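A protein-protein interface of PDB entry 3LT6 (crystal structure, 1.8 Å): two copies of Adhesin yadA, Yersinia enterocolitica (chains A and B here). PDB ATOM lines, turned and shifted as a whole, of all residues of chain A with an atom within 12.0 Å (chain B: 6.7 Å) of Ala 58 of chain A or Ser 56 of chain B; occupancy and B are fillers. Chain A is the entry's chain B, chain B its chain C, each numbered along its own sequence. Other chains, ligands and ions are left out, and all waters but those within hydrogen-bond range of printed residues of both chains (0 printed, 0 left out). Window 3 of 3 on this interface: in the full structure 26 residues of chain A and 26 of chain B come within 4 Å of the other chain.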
ATOM      1  N   ARG A  49     -37.379  26.570   6.458  1.00  0.00           N
ATOM      2  CA  ARG A  49     -36.119  27.365   6.522  1.00  0.00           C
ATOM      3  C   ARG A  49     -35.016  26.584   5.862  1.00  0.00           C
ATOM      4  O   ARG A  49     -34.350  27.104   4.971  1.00  0.00           O
ATOM      5  CB  ARG A  49     -35.704  27.745   7.942  1.00  0.00           C
ATOM      6  CG  ARG A  49     -34.706  28.932   7.978  1.00  0.00           C
ATOM      7  CD  ARG A  49     -34.387  29.403   9.419  1.00  0.00           C
ATOM      8  NE  ARG A  49     -35.585  29.326  10.256  1.00  0.00           N
ATOM      9  CZ  ARG A  49     -36.564  30.234  10.247  1.00  0.00           C
ATOM     10  NH1 ARG A  49     -36.482  31.312   9.459  1.00  0.00           N
ATOM     11  NH2 ARG A  49     -37.631  30.070  11.029  1.00  0.00           N
ATOM     12  N   LEU A  50     -34.818  25.331   6.276  1.00  0.00           N
ATOM     13  CA  LEU A  50     -33.820  24.498   5.592  1.00  0.00           C
ATOM     14  C   LEU A  50     -33.952  24.395   4.047  1.00  0.00           C
ATOM     15  O   LEU A  50     -32.989  24.588   3.316  1.00  0.00           O
ATOM     16  CB  LEU A  50     -33.795  23.114   6.198  1.00  0.00           C
ATOM     17  CG  LEU A  50     -32.943  22.956   7.414  1.00  0.00           C
ATOM     18  CD1 LEU A  50     -33.173  21.548   7.923  1.00  0.00           C
ATOM     19  CD2 LEU A  50     -31.553  23.123   7.055  1.00  0.00           C
ATOM     20  N   LEU A  51     -35.131  24.055   3.540  1.00  0.00           N
ATOM     21  CA  LEU A  51     -35.312  24.065   2.094  1.00  0.00           C
ATOM     22  C   LEU A  51     -34.921  25.375   1.454  1.00  0.00           C
ATOM     23  O   LEU A  51     -34.310  25.383   0.356  1.00  0.00           O
ATOM     24  CB  LEU A  51     -36.739  23.686   1.728  1.00  0.00           C
ATOM     25  CG  LEU A  51     -37.176  22.229   1.725  1.00  0.00           C
ATOM     26  CD1 LEU A  51     -36.983  21.458   3.057  1.00  0.00           C
ATOM     27  CD2 LEU A  51     -38.665  22.263   1.454  1.00  0.00           C
ATOM     28  N   LYS A  52     -35.225  26.486   2.124  1.00  0.00           N
ATOM     29  CA  LYS A  52     -34.848  27.807   1.611  1.00  0.00           C
ATOM     30  C   LYS A  52     -33.325  27.964   1.644  1.00  0.00           C
ATOM     31  O   LYS A  52     -32.767  28.303   0.645  1.00  0.00           O
ATOM     32  CB  LYS A  52     -35.487  28.957   2.398  1.00  0.00           C
ATOM     33  CG  LYS A  52     -37.003  29.010   2.383  1.00  0.00           C
ATOM     34  CD  LYS A  52     -37.538  29.712   3.670  1.00  0.00           C
ATOM     35  CE  LYS A  52     -39.025  29.465   3.866  1.00  0.00           C
ATOM     36  NZ  LYS A  52     -39.785  29.951   2.676  1.00  0.00           N
ATOM     37  N   LEU A  53     -32.673  27.671   2.774  1.00  0.00           N
ATOM     38  CA  LEU A  53     -31.206  27.812   2.866  1.00  0.00           C
ATOM     39  C   LEU A  53     -30.495  26.871   1.910  1.00  0.00           C
ATOM     40  O   LEU A  53     -29.491  27.216   1.349  1.00  0.00           O
ATOM     41  CB  LEU A  53     -30.713  27.559   4.291  1.00  0.00           C
ATOM     42  CG  LEU A  53     -31.152  28.558   5.360  1.00  0.00           C
ATOM     43  CD1 LEU A  53     -30.767  28.032   6.704  1.00  0.00           C
ATOM     44  CD2 LEU A  53     -30.508  29.884   5.110  1.00  0.00           C
ATOM     45  N   LEU A  54     -31.012  25.654   1.751  1.00  0.00           N
ATOM     46  CA  LEU A  54     -30.413  24.732   0.794  1.00  0.00           C
ATOM     47  C   LEU A  54     -30.460  25.219  -0.651  1.00  0.00           C
ATOM     48  O   LEU A  54     -29.462  25.102  -1.376  1.00  0.00           O
ATOM     49  CB  LEU A  54     -31.066  23.364   0.876  1.00  0.00           C
ATOM     50  CG  LEU A  54     -30.614  22.451   1.986  1.00  0.00           C
ATOM     51  CD1 LEU A  54     -31.783  21.453   2.264  1.00  0.00           C
ATOM     52  CD2 LEU A  54     -29.406  21.656   1.613  1.00  0.00           C
ATOM     53  N   ALA A  55     -31.604  25.742  -1.087  1.00  0.00           N
ATOM     54  CA  ALA A  55     -31.714  26.235  -2.462  1.00  0.00           C
ATOM     55  C   ALA A  55     -30.891  27.485  -2.725  1.00  0.00           C
ATOM     56  O   ALA A  55     -30.330  27.648  -3.824  1.00  0.00           O
ATOM     57  CB  ALA A  55     -33.192  26.451  -2.842  1.00  0.00           C
ATOM     58  N   SER A  56     -30.756  28.385  -1.751  1.00  0.00           N
ATOM     59  CA  SER A  56     -29.919  29.551  -2.052  1.00  0.00           C
ATOM     60  C   SER A  56     -28.395  29.287  -1.970  1.00  0.00           C
ATOM     61  O   SER A  56     -27.600  29.936  -2.658  1.00  0.00           O
ATOM     62  CB  SER A  56     -30.339  30.806  -1.294  1.00  0.00           C
ATOM     63  OG  SER A  56     -30.297  30.619   0.088  1.00  0.00           O
ATOM     64  N   SER A  57     -28.002  28.312  -1.157  1.00  0.00           N
ATOM     65  CA  SER A  57     -26.619  27.855  -1.160  1.00  0.00           C
ATOM     66  C   SER A  57     -26.331  26.983  -2.380  1.00  0.00           C
ATOM     67  O   SER A  57     -25.265  27.091  -2.965  1.00  0.00           O
ATOM     68  CB  SER A  57     -26.264  27.111   0.123  1.00  0.00           C
ATOM     69  OG  SER A  57     -26.993  25.900   0.214  1.00  0.00           O
ATOM     70  N   ALA A  58     -27.277  26.116  -2.740  1.00  0.00           N
ATOM     71  CA  ALA A  58     -27.152  25.285  -3.931  1.00  0.00           C
ATOM     72  C   ALA A  58     -27.166  26.145  -5.191  1.00  0.00           C
ATOM     73  O   ALA A  58     -26.490  25.810  -6.163  1.00  0.00           O
ATOM     74  CB  ALA A  58     -28.246  24.220  -3.985  1.00  0.00           C
ATOM     75  N   ALA A  59     -27.929  27.247  -5.161  1.00  0.00           N
ATOM     76  CA  ALA A  59     -27.803  28.313  -6.196  1.00  0.00           C
ATOM     77  C   ALA A  59     -26.441  29.034  -6.202  1.00  0.00           C
ATOM     78  O   ALA A  59     -25.782  29.079  -7.247  1.00  0.00           O
ATOM     79  CB  ALA A  59     -28.971  29.339  -6.126  1.00  0.00           C
ATOM     80  N   LEU A  60     -26.018  29.618  -5.083  1.00  0.00           N
ATOM     81  CA  LEU A  60     -24.683  30.236  -5.017  1.00  0.00           C
ATOM     82  C   LEU A  60     -23.523  29.368  -5.536  1.00  0.00           C
ATOM     83  O   LEU A  60     -22.628  29.875  -6.219  1.00  0.00           O
ATOM     84  CB  LEU A  60     -24.377  30.767  -3.616  1.00  0.00           C
ATOM     85  CG  LEU A  60     -24.393  32.287  -3.541  1.00  0.00           C
ATOM     86  CD1 LEU A  60     -23.525  32.768  -2.391  1.00  0.00           C
ATOM     87  CD2 LEU A  60     -23.839  32.793  -4.838  1.00  0.00           C
ATOM     88  N   ASN A  61     -23.539  28.073  -5.208  1.00  0.00           N
ATOM     89  CA  ASN A  61     -22.514  27.112  -5.685  1.00  0.00           C
ATOM     90  C   ASN A  61     -22.466  27.038  -7.218  1.00  0.00           C
ATOM     91  O   ASN A  61     -21.398  27.134  -7.824  1.00  0.00           O
ATOM     92  CB  ASN A  61     -22.723  25.698  -5.095  1.00  0.00           C
ATOM     93  CG  ASN A  61     -22.089  25.523  -3.706  1.00  0.00           C
ATOM     94  OD1 ASN A  61     -20.860  25.497  -3.559  1.00  0.00           O
ATOM     95  ND2 ASN A  61     -22.927  25.379  -2.687  1.00  0.00           N
ATOM     96  N   SER A  62     -23.644  26.861  -7.819  1.00  0.00           N
ATOM     97  CA  SER A  62     -23.827  26.785  -9.275  1.00  0.00           C
ATOM     98  C   SER A  62     -23.375  28.042  -9.992  1.00  0.00           C
ATOM     99  O   SER A  62     -22.707  27.963 -11.022  1.00  0.00           O
ATOM    100  CB  SER A  62     -25.313  26.566  -9.574  1.00  0.00           C
ATOM    101  OG  SER A  62     -26.068  27.676  -9.095  1.00  0.00           O
ATOM    102  N   LEU A  63     -23.763  29.195  -9.454  1.00  0.00           N
ATOM    103  CA  LEU A  63     -23.379  30.480 -10.008  1.00  0.00           C
ATOM    104  C   LEU A  63     -21.854  30.594  -9.973  1.00  0.00           C
ATOM    105  O   LEU A  63     -21.221  30.701 -11.032  1.00  0.00           O
ATOM    106  CB  LEU A  63     -24.055  31.635  -9.252  1.00  0.00           C
ATOM    107  CG  LEU A  63     -25.465  32.050  -9.679  1.00  0.00           C
ATOM    108  CD1 LEU A  63     -26.428  32.165  -8.498  1.00  0.00           C
ATOM    109  CD2 LEU A  63     -25.438  33.366 -10.480  1.00  0.00           C
ATOM    110  N   PHE A  64     -21.273  30.561  -8.771  1.00  0.00           N
ATOM    111  CA  PHE A  64     -19.818  30.450  -8.584  1.00  0.00           C
ATOM    112  C   PHE A  64     -19.363  29.117  -9.126  1.00  0.00           C
ATOM    113  O   PHE A  64     -18.774  29.044 -10.187  1.00  0.00           O
ATOM    114  CB  PHE A  64     -19.474  30.544  -7.101  1.00  0.00           C
ATOM    115  N   LEU B  51     -27.419  18.168   7.230  1.00  0.00           N
ATOM    116  CA  LEU B  51     -26.120  17.611   6.802  1.00  0.00           C
ATOM    117  C   LEU B  51     -25.807  18.034   5.357  1.00  0.00           C
ATOM    118  O   LEU B  51     -24.654  18.385   5.025  1.00  0.00           O
ATOM    119  CB  LEU B  51     -26.089  16.078   7.035  1.00  0.00           C
ATOM    120  CG  LEU B  51     -25.979  15.688   8.539  1.00  0.00           C
ATOM    121  CD1 LEU B  51     -26.323  14.180   8.875  1.00  0.00           C
ATOM    122  CD2 LEU B  51     -24.640  16.022   9.128  1.00  0.00           C
ATOM    123  N   LYS B  52     -26.838  18.093   4.529  1.00  0.00           N
ATOM    124  CA  LYS B  52     -26.636  18.653   3.190  1.00  0.00           C
ATOM    125  C   LYS B  52     -26.161  20.110   3.173  1.00  0.00           C
ATOM    126  O   LYS B  52     -25.165  20.437   2.481  1.00  0.00           O
ATOM    127  CB  LYS B  52     -27.841  18.460   2.293  1.00  0.00           C
ATOM    128  CG  LYS B  52     -27.504  18.781   0.802  1.00  0.00           C
ATOM    129  CD  LYS B  52     -28.318  17.882  -0.097  1.00  0.00           C
ATOM    130  CE  LYS B  52     -28.467  18.476  -1.495  1.00  0.00           C
ATOM    131  NZ  LYS B  52     -29.145  17.507  -2.435  1.00  0.00           N
ATOM    132  N   LEU B  53     -26.883  20.958   3.890  1.00  0.00           N
ATOM    133  CA  LEU B  53     -26.567  22.379   3.986  1.00  0.00           C
ATOM    134  C   LEU B  53     -25.178  22.614   4.558  1.00  0.00           C
ATOM    135  O   LEU B  53     -24.469  23.491   4.089  1.00  0.00           O
ATOM    136  CB  LEU B  53     -27.614  23.108   4.830  1.00  0.00           C
ATOM    137  CG  LEU B  53     -27.353  24.591   5.119  1.00  0.00           C
ATOM    138  CD1 LEU B  53     -27.490  25.332   3.816  1.00  0.00           C
ATOM    139  CD2 LEU B  53     -28.359  25.037   6.136  1.00  0.00           C
ATOM    140  N   LEU B  54     -24.822  21.878   5.605  1.00  0.00           N
ATOM    141  CA  LEU B  54     -23.455  21.885   6.122  1.00  0.00           C
ATOM    142  C   LEU B  54     -22.383  21.752   5.033  1.00  0.00           C
ATOM    143  O   LEU B  54     -21.451  22.581   4.944  1.00  0.00           O
ATOM    144  CB  LEU B  54     -23.231  20.765   7.139  1.00  0.00           C
ATOM    145  CG  LEU B  54     -23.123  21.047   8.630  1.00  0.00           C
ATOM    146  CD1 LEU B  54     -22.772  19.706   9.342  1.00  0.00           C
ATOM    147  CD2 LEU B  54     -22.115  22.132   9.031  1.00  0.00           C
ATOM    148  N   ALA B  55     -22.483  20.710   4.223  1.00  0.00           N
ATOM    149  CA  ALA B  55     -21.464  20.495   3.205  1.00  0.00           C
ATOM    150  C   ALA B  55     -21.530  21.579   2.153  1.00  0.00           C
ATOM    151  O   ALA B  55     -20.520  22.014   1.597  1.00  0.00           O
ATOM    152  CB  ALA B  55     -21.665  19.139   2.556  1.00  0.00           C
ATOM    153  N   SER B  56     -22.756  21.936   1.826  1.00  0.00           N
ATOM    154  CA  SER B  56     -23.013  22.967   0.846  1.00  0.00           C
ATOM    155  C   SER B  56     -22.389  24.299   1.305  1.00  0.00           C
ATOM    156  O   SER B  56     -21.793  25.021   0.511  1.00  0.00           O
ATOM    157  CB  SER B  56     -24.535  23.046   0.627  1.00  0.00           C
ATOM    158  OG  SER B  56     -24.861  24.011  -0.348  1.00  0.00           O
ATOM    159  N   SER B  57     -22.481  24.602   2.603  1.00  0.00           N
ATOM    160  CA  SER B  57     -21.960  25.837   3.143  1.00  0.00           C
ATOM    161  C   SER B  57     -20.444  25.872   3.037  1.00  0.00           C
ATOM    162  O   SER B  57     -19.856  26.909   2.614  1.00  0.00           O
ATOM    163  CB  SER B  57     -22.409  26.024   4.598  1.00  0.00           C
ATOM    164  OG  SER B  57     -21.873  27.231   5.109  1.00  0.00           O
ATOM    165  N   ALA B  58     -19.820  24.744   3.387  1.00  0.00           N
ATOM    166  CA  ALA B  58     -18.354  24.616   3.387  1.00  0.00           C
ATOM    167  C   ALA B  58     -17.839  24.648   1.963  1.00  0.00           C
ATOM    168  O   ALA B  58     -16.698  25.065   1.727  1.00  0.00           O
ATOM    169  CB  ALA B  58     -17.918  23.305   4.083  1.00  0.00           C
ATOM    170  N   ALA B  59     -18.683  24.209   1.025  1.00  0.00           N
ATOM    171  CA  ALA B  59     -18.355  24.218  -0.411  1.00  0.00           C
ATOM    172  C   ALA B  59     -18.434  25.616  -1.002  1.00  0.00           C
ATOM    173  O   ALA B  59     -17.590  25.990  -1.860  1.00  0.00           O
ATOM    174  CB  ALA B  59     -19.242  23.247  -1.174  1.00  0.00           C
ATOM    175  N   LEU B  60     -19.414  26.389  -0.537  1.00  0.00           N
ATOM    176  CA  LEU B  60     -19.500  27.808  -0.808  1.00  0.00           C
ATOM    177  C   LEU B  60     -18.275  28.633  -0.423  1.00  0.00           C
ATOM    178  O   LEU B  60     -18.230  29.825  -0.725  1.00  0.00           O
ATOM    179  CB  LEU B  60     -20.749  28.416  -0.173  1.00  0.00           C
ATOM    180  CG  LEU B  60     -21.751  28.968  -1.168  1.00  0.00           C
ATOM    181  CD1 LEU B  60     -23.106  29.252  -0.499  1.00  0.00           C
ATOM    182  CD2 LEU B  60     -21.208  30.236  -1.860  1.00  0.00           C
ATOM    183  N   ASN B  61     -17.271  28.013   0.211  1.00  0.00           N
ATOM    184  CA  ASN B  61     -15.954  28.659   0.409  1.00  0.00           C
ATOM    185  C   ASN B  61     -14.793  27.802  -0.164  1.00  0.00           C
ATOM    186  O   ASN B  61     -14.551  26.709   0.346  1.00  0.00           O
ATOM    187  CB  ASN B  61     -15.687  28.986   1.902  1.00  0.00           C
ATOM    188  CG  ASN B  61     -16.951  28.929   2.783  1.00  0.00           C
ATOM    189  OD1 ASN B  61     -17.356  29.923   3.402  1.00  0.00           O
ATOM    190  ND2 ASN B  61     -17.547  27.757   2.866  1.00  0.00           N
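OD1 of Asn 61 of chain A lies within hydrogen-bond range of N of Leu 60 of chain B, 3.5 Å away. The side-chain hydroxyl (OG) of Ser 57 of chain A sits at hydrogen-bond distance from the side-chain hydroxyl (OG) of Ser 56 of chain B. The side-chain hydroxyl (OG) of Ser 56 of chain B sits at hydrogen-bond distance from the side-chain amide nitrogen (ND2) of Asn 61 of chain A, 3.3 Å away.
ND2 of Asn 61 of chain A is in hydrogen-bond range of O of Ser 57 of chain A, at 2.9 Å. O of Leu 53 of chain A is in hydrogen-bond range of OG of Ser 57 of chain A, at 3.0 Å. The side-chain hydroxyl (OG) of Ser 57 of chain A lies within hydrogen-bond range of the backbone carbonyl oxygen (O) of Leu 54 of chain A.
Among the printed residues, merely in contact across the chains: Leu 50 of chain A with Leu 53 of chain B (3.8 Å), Leu 53 of chain A with Leu 53 of chain B (3.7 Å), Leu 54 of chain A with Lys 52 of chain B (3.5 Å), Leu 54 of chain A with Leu 53 of chain B (3.5 Å), Ser 57 of chain A with Leu 53 of chain B (3.7 Å), Ser 57 of chain A with Leu 60 of chain B (3.8 Å), Ala 58 of chain A with Ser 56 of chain B (3.999 Å), Leu 60 of chain A with Leu 60 of chain B (3.5 Å) and Asn 61 of chain A with Ala 59 of chain B (3.5 Å).
Printed residues of chain B within 4 Å of Leu 53 of chain A: Leu 53. Of the printed residues of chain B, Leu 54 of chain A touches Lys 52 (3.5 Å) and Leu 53 (3.5 Å). Printed residues of chain B within 4 Å of Ala 58 of chain A: Ser 56. Printed residues of chain B within 4 Å of Leu 60 of chain A: Leu 60 (3.5 Å). Printed residues of chain B within 4 Å of Asn 61 of chain A: Ser 56 (3.3 Å), Ala 59 (3.5 Å) and Leu 60 (3.5 Å). Leu 63 of chain A touches none of the printed residues of chain B. No residue of chain A comes within 4 Å of Leu 54 of chain B. Of the printed residues of chain A, Ser 56 of chain B touches Ser 57, Ala 58 and Asn 61. Ala 59 of chain B touches just one residue of chain A: Asn 61. Leu 60 of chain B touches three residues of chain A. The nearest printed residue of chain A that does not touch Ser 56 of chain B is Leu 54 of chain A (4.8 Å). The nearest printed residue of chain B that does not touch Leu 54 of chain A is Ser 56 of chain B (4.8 Å).
Printed residues of chain B that touch a printed residue of chain A: Lys 52, Leu 53, Ser 56, Ala 59 and Leu 60. Hydrophobic or aromatic side chains of chain B within 4 Å of the printed part of chain A: Leu 53, Ala 59 and Leu 60. Along chain A the printed residues that touch a printed residue of chain B span positions 50 to 61. Among the printed residues, 12 pairs touch across the chains.
Leu 53 of chain A touches its own counterpart, Leu 53 of chain B. Leu 54 of chain A touches Leu 53 of chain B, but with the chains exchanged Leu 53 of chain A does not touch Leu 54 of chain B (8.3 Å). Ser 57 of chain A touches Ser 56 of chain B, but with the chains exchanged Ser 56 of chain A does not touch Ser 57 of chain B (8.8 Å). Asn 61 of chain A touches Leu 60 of chain B, but with the chains exchanged Leu 60 of chain A does not touch Asn 61 of chain B (8.3 Å). 11 positions are printed for both chains.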
